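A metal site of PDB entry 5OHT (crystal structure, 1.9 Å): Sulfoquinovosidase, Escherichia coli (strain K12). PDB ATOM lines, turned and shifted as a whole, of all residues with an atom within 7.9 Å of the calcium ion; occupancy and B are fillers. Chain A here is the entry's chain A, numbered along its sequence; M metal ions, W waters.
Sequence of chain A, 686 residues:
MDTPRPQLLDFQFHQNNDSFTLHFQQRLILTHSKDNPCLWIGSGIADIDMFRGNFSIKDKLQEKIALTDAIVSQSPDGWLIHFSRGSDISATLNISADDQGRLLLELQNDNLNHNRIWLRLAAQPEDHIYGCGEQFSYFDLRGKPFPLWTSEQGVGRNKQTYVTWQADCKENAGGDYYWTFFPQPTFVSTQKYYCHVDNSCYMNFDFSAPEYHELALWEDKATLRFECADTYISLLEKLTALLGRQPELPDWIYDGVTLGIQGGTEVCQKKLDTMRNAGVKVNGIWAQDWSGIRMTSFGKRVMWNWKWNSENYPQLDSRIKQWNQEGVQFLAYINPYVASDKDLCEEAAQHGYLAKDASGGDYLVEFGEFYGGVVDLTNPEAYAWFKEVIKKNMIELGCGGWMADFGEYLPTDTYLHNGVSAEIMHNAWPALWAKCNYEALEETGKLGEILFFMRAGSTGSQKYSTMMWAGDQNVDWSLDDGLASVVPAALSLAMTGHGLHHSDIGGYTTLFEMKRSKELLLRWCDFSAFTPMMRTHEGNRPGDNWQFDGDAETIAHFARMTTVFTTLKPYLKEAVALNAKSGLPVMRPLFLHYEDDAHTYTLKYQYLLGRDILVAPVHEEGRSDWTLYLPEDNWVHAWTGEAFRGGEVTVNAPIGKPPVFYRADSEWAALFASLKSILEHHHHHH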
ATOM      1  N   PHE A 136      31.629 -18.126  -5.659  1.00  0.00           N
ATOM      2  CA  PHE A 136      31.148 -16.994  -4.873  1.00  0.00           C
ATOM      3  C   PHE A 136      32.151 -16.466  -3.852  1.00  0.00           C
ATOM      4  O   PHE A 136      31.959 -15.307  -3.386  1.00  0.00           O
ATOM      5  CB  PHE A 136      29.833 -17.360  -4.137  1.00  0.00           C
ATOM      6  CG  PHE A 136      28.632 -17.522  -5.042  1.00  0.00           C
ATOM      7  CD1 PHE A 136      28.358 -18.737  -5.644  1.00  0.00           C
ATOM      8  CD2 PHE A 136      27.705 -16.500  -5.190  1.00  0.00           C
ATOM      9  CE1 PHE A 136      27.208 -18.968  -6.403  1.00  0.00           C
ATOM     10  CE2 PHE A 136      26.578 -16.686  -5.943  1.00  0.00           C
ATOM     11  CZ  PHE A 136      26.307 -17.923  -6.576  1.00  0.00           C
ATOM     12  N   GLU A 152      22.585 -27.128  -2.904  1.00  0.00           N
ATOM     13  CA  GLU A 152      22.313 -25.886  -2.210  1.00  0.00           C
ATOM     14  C   GLU A 152      23.661 -25.152  -1.990  1.00  0.00           C
ATOM     15  O   GLU A 152      24.713 -25.789  -1.740  1.00  0.00           O
ATOM     16  CB  GLU A 152      21.600 -26.135  -0.882  1.00  0.00           C
ATOM     17  CG  GLU A 152      20.114 -26.236  -1.075  1.00  0.00           C
ATOM     18  CD  GLU A 152      19.406 -24.885  -1.417  1.00  0.00           C
ATOM     19  OE1 GLU A 152      20.040 -23.791  -1.333  1.00  0.00           O
ATOM     20  OE2 GLU A 152      18.200 -24.955  -1.777  1.00  0.00           O
ATOM     21  N   GLN A 153      23.594 -23.830  -2.008  1.00  0.00           N
ATOM     22  CA  GLN A 153      24.843 -22.971  -2.091  1.00  0.00           C
ATOM     23  C   GLN A 153      25.422 -22.568  -0.753  1.00  0.00           C
ATOM     24  O   GLN A 153      26.552 -22.092  -0.639  1.00  0.00           O
ATOM     25  CB  GLN A 153      24.512 -21.754  -3.009  1.00  0.00           C
ATOM     26  CG  GLN A 153      25.622 -20.743  -3.302  1.00  0.00           C
ATOM     27  CD  GLN A 153      25.457 -19.426  -2.571  1.00  0.00           C
ATOM     28  OE1 GLN A 153      24.659 -19.302  -1.615  1.00  0.00           O
ATOM     29  NE2 GLN A 153      26.225 -18.416  -2.990  1.00  0.00           N
ATOM     30  N   GLY A 154      24.626 -22.789   0.307  1.00  0.00           N
ATOM     31  CA  GLY A 154      24.985 -22.500   1.663  1.00  0.00           C
ATOM     32  C   GLY A 154      24.353 -21.190   2.216  1.00  0.00           C
ATOM     33  O   GLY A 154      24.117 -20.209   1.456  1.00  0.00           O
ATOM     34  N   VAL A 155      24.141 -21.163   3.533  1.00  0.00           N
ATOM     35  CA  VAL A 155      23.688 -19.946   4.234  1.00  0.00           C
ATOM     36  C   VAL A 155      24.824 -19.500   5.133  1.00  0.00           C
ATOM     37  O   VAL A 155      25.132 -20.154   6.178  1.00  0.00           O
ATOM     38  CB  VAL A 155      22.432 -20.226   5.077  1.00  0.00           C
ATOM     39  CG1 VAL A 155      22.046 -19.013   5.918  1.00  0.00           C
ATOM     40  CG2 VAL A 155      21.333 -20.732   4.197  1.00  0.00           C
ATOM     41  N   GLY A 156      25.462 -18.395   4.754  1.00  0.00           N
ATOM     42  CA  GLY A 156      26.692 -17.932   5.388  1.00  0.00           C
ATOM     43  C   GLY A 156      28.006 -18.375   4.704  1.00  0.00           C
ATOM     44  O   GLY A 156      28.923 -17.545   4.467  1.00  0.00           O
ATOM     45  N   ARG A 157      28.144 -19.684   4.430  1.00  0.00           N
ATOM     46  CA  ARG A 157      29.259 -20.249   3.595  1.00  0.00           C
ATOM     47  C   ARG A 157      30.711 -20.051   4.150  1.00  0.00           C
ATOM     48  O   ARG A 157      31.677 -20.231   3.400  1.00  0.00           O
ATOM     49  CB  ARG A 157      29.176 -19.654   2.141  1.00  0.00           C
ATOM     50  CG  ARG A 157      27.779 -19.707   1.538  1.00  0.00           C
ATOM     51  CD  ARG A 157      27.705 -19.246   0.077  1.00  0.00           C
ATOM     52  NE  ARG A 157      28.573 -20.022  -0.799  1.00  0.00           N
ATOM     53  CZ  ARG A 157      29.846 -19.728  -1.123  1.00  0.00           C
ATOM     54  NH1 ARG A 157      30.414 -18.604  -0.726  1.00  0.00           N
ATOM     55  NH2 ARG A 157      30.527 -20.555  -1.901  1.00  0.00           N
ATOM     56  N   ALA A 173      23.481 -27.015   6.827  1.00  0.00           N
ATOM     57  CA  ALA A 173      23.063 -25.901   5.857  1.00  0.00           C
ATOM     58  C   ALA A 173      24.015 -24.661   5.690  1.00  0.00           C
ATOM     59  O   ALA A 173      23.820 -23.886   4.765  1.00  0.00           O
ATOM     60  CB  ALA A 173      21.639 -25.400   6.163  1.00  0.00           C
ATOM     61  N   GLY A 174      25.005 -24.500   6.532  1.00  0.00           N
ATOM     62  CA  GLY A 174      25.928 -23.346   6.461  1.00  0.00           C
ATOM     63  C   GLY A 174      26.825 -23.361   5.210  1.00  0.00           C
ATOM     64  O   GLY A 174      27.153 -22.298   4.651  1.00  0.00           O
ATOM     65  N   PHE A 181      25.370 -23.628  -6.812  1.00  0.00           N
ATOM     66  CA  PHE A 181      24.342 -24.127  -7.685  1.00  0.00           C
ATOM     67  C   PHE A 181      24.893 -24.521  -9.093  1.00  0.00           C
ATOM     68  O   PHE A 181      24.227 -25.272  -9.814  1.00  0.00           O
ATOM     69  CB  PHE A 181      23.190 -23.122  -7.889  1.00  0.00           C
ATOM     70  CG  PHE A 181      22.742 -22.346  -6.671  1.00  0.00           C
ATOM     71  CD1 PHE A 181      21.894 -22.917  -5.727  1.00  0.00           C
ATOM     72  CD2 PHE A 181      23.103 -21.013  -6.501  1.00  0.00           C
ATOM     73  CE1 PHE A 181      21.422 -22.161  -4.639  1.00  0.00           C
ATOM     74  CE2 PHE A 181      22.688 -20.280  -5.399  1.00  0.00           C
ATOM     75  CZ  PHE A 181      21.814 -20.861  -4.492  1.00  0.00           C
ATOM     76  N   ALA A 470      22.153 -14.836  -9.544  1.00  0.00           N
ATOM     77  CA  ALA A 470      23.106 -15.286  -8.535  1.00  0.00           C
ATOM     78  C   ALA A 470      22.488 -16.156  -7.389  1.00  0.00           C
ATOM     79  O   ALA A 470      23.125 -16.475  -6.427  1.00  0.00           O
ATOM     80  CB  ALA A 470      23.865 -14.103  -7.957  1.00  0.00           C
ATOM     81  N   GLY A 471      21.251 -16.593  -7.530  1.00  0.00           N
ATOM     82  CA  GLY A 471      20.567 -17.360  -6.514  1.00  0.00           C
ATOM     83  C   GLY A 471      20.346 -16.630  -5.189  1.00  0.00           C
ATOM     84  O   GLY A 471      20.219 -15.456  -5.201  1.00  0.00           O
ATOM     85  N   ASP A 472      20.401 -17.385  -4.062  1.00  0.00           N
ATOM     86  CA  ASP A 472      20.076 -16.857  -2.732  1.00  0.00           C
ATOM     87  C   ASP A 472      21.317 -16.318  -1.941  1.00  0.00           C
ATOM     88  O   ASP A 472      22.145 -17.099  -1.436  1.00  0.00           O
ATOM     89  CB  ASP A 472      19.411 -17.930  -1.814  1.00  0.00           C
ATOM     90  CG  ASP A 472      18.167 -18.601  -2.451  1.00  0.00           C
ATOM     91  OD1 ASP A 472      17.774 -18.306  -3.620  1.00  0.00           O
ATOM     92  OD2 ASP A 472      17.592 -19.442  -1.758  1.00  0.00           O
ATOM     93  N   GLN A 473      21.438 -14.997  -1.861  1.00  0.00           N
ATOM     94  CA  GLN A 473      22.326 -14.296  -0.920  1.00  0.00           C
ATOM     95  C   GLN A 473      21.538 -14.050   0.357  1.00  0.00           C
ATOM     96  O   GLN A 473      20.286 -13.931   0.336  1.00  0.00           O
ATOM     97  CB  GLN A 473      22.794 -12.906  -1.413  1.00  0.00           C
ATOM     98  CG  GLN A 473      23.896 -12.910  -2.490  1.00  0.00           C
ATOM     99  CD  GLN A 473      23.381 -13.470  -3.812  1.00  0.00           C
ATOM    100  OE1 GLN A 473      22.519 -12.861  -4.490  1.00  0.00           O
ATOM    101  NE2 GLN A 473      23.874 -14.682  -4.173  1.00  0.00           N
ATOM    102  N   ASN A 474      22.256 -14.037   1.473  1.00  0.00           N
ATOM    103  CA  ASN A 474      21.670 -13.486   2.749  1.00  0.00           C
ATOM    104  C   ASN A 474      21.339 -12.016   2.583  1.00  0.00           C
ATOM    105  O   ASN A 474      21.958 -11.309   1.736  1.00  0.00           O
ATOM    106  CB  ASN A 474      22.663 -13.601   3.933  1.00  0.00           C
ATOM    107  CG  ASN A 474      22.983 -15.003   4.322  1.00  0.00           C
ATOM    108  OD1 ASN A 474      22.261 -15.949   3.969  1.00  0.00           O
ATOM    109  ND2 ASN A 474      24.070 -15.161   5.086  1.00  0.00           N
ATOM    110  N   ASP A 480      31.129 -13.548   1.950  1.00  0.00           N
ATOM    111  CA  ASP A 480      30.849 -14.863   1.356  1.00  0.00           C
ATOM    112  C   ASP A 480      29.401 -15.121   0.956  1.00  0.00           C
ATOM    113  O   ASP A 480      29.157 -16.081   0.186  1.00  0.00           O
ATOM    114  CB  ASP A 480      31.392 -16.002   2.275  1.00  0.00           C
ATOM    115  CG  ASP A 480      32.945 -15.946   2.422  1.00  0.00           C
ATOM    116  OD1 ASP A 480      33.654 -16.306   1.455  1.00  0.00           O
ATOM    117  OD2 ASP A 480      33.450 -15.465   3.464  1.00  0.00           O
ATOM    118  N   ASP A 481      28.417 -14.414   1.526  1.00  0.00           N
ATOM    119  CA  ASP A 481      27.016 -14.688   1.149  1.00  0.00           C
ATOM    120  C   ASP A 481      26.126 -13.405   1.102  1.00  0.00           C
ATOM    121  O   ASP A 481      24.930 -13.522   1.074  1.00  0.00           O
ATOM    122  CB  ASP A 481      26.408 -15.769   2.080  1.00  0.00           C
ATOM    123  CG  ASP A 481      25.327 -16.644   1.432  1.00  0.00           C
ATOM    124  OD1 ASP A 481      25.047 -16.674   0.209  1.00  0.00           O
ATOM    125  OD2 ASP A 481      24.704 -17.405   2.165  1.00  0.00           O
ATOM    126  N   GLY A 482      26.755 -12.221   1.081  1.00  0.00           N
ATOM    127  CA  GLY A 482      26.064 -10.971   0.919  1.00  0.00           C
ATOM    128  C   GLY A 482      26.208 -10.366  -0.447  1.00  0.00           C
ATOM    129  O   GLY A 482      26.586 -11.043  -1.424  1.00  0.00           O
ATOM    130  N   SER A 485      29.473 -11.020  -2.687  1.00  0.00           N
ATOM    131  CA  SER A 485      29.611 -12.343  -3.280  1.00  0.00           C
ATOM    132  C   SER A 485      29.096 -12.415  -4.716  1.00  0.00           C
ATOM    133  O   SER A 485      29.481 -13.349  -5.464  1.00  0.00           O
ATOM    134  CB  SER A 485      28.965 -13.386  -2.388  1.00  0.00           C
ATOM    135  OG  SER A 485      27.548 -13.347  -2.389  1.00  0.00           O
ATOM    136  N   TYR A 508      17.923 -12.308  -0.560  1.00  0.00           N
ATOM    137  CA  TYR A 508      16.806 -13.236  -0.331  1.00  0.00           C
ATOM    138  C   TYR A 508      16.664 -13.812   1.077  1.00  0.00           C
ATOM    139  O   TYR A 508      15.586 -13.652   1.726  1.00  0.00           O
ATOM    140  CB  TYR A 508      16.897 -14.396  -1.307  1.00  0.00           C
ATOM    141  CG  TYR A 508      15.784 -15.410  -1.118  1.00  0.00           C
ATOM    142  CD1 TYR A 508      14.476 -15.100  -1.494  1.00  0.00           C
ATOM    143  CD2 TYR A 508      16.029 -16.656  -0.489  1.00  0.00           C
ATOM    144  CE1 TYR A 508      13.458 -16.003  -1.261  1.00  0.00           C
ATOM    145  CE2 TYR A 508      14.979 -17.579  -0.295  1.00  0.00           C
ATOM    146  CZ  TYR A 508      13.712 -17.228  -0.650  1.00  0.00           C
ATOM    147  OH  TYR A 508      12.690 -18.133  -0.460  1.00  0.00           O
ATOM    148  N   THR A 509      17.711 -14.479   1.563  1.00  0.00           N
ATOM    149  CA  THR A 509      17.606 -15.362   2.743  1.00  0.00           C
ATOM    150  C   THR A 509      17.460 -14.575   4.066  1.00  0.00           C
ATOM    151  O   THR A 509      18.365 -13.831   4.444  1.00  0.00           O
ATOM    152  CB  THR A 509      18.802 -16.316   2.835  1.00  0.00           C
ATOM    153  OG1 THR A 509      19.006 -17.017   1.567  1.00  0.00           O
ATOM    154  CG2 THR A 509      18.504 -17.339   3.998  1.00  0.00           C
HETATM  155 CA    CA M   1      23.398 -18.379   0.163  1.00  0.00          CA
HETATM  156  O   HOH W   1      21.830 -20.132  -0.162  1.00  0.00           O
HETATM  157  O   HOH W   2      21.686 -17.539   1.757  1.00  0.00           O
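The guanidinium group (NE) of Arg 157 lies within hydrogen-bond range of the backbone carbonyl oxygen (O) of Gln 153 (2.9 Å).
The backbone carbonyl oxygen (O) of Asp 481 lies within hydrogen-bond range of the backbone NH (N) of Asn 474.
OD2 of Asp 481 sits close to N of Gly 156 (2.9 Å).
The calcium ion is bound by O of Gly 154, OE1 of Gln 153, OD1 of Asp 481, water W1, O of Asp 472, water W2 and OD2 of Asp 481.
Water W2 bridges OG1 of Thr 509 and OD1 of Asn 474.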
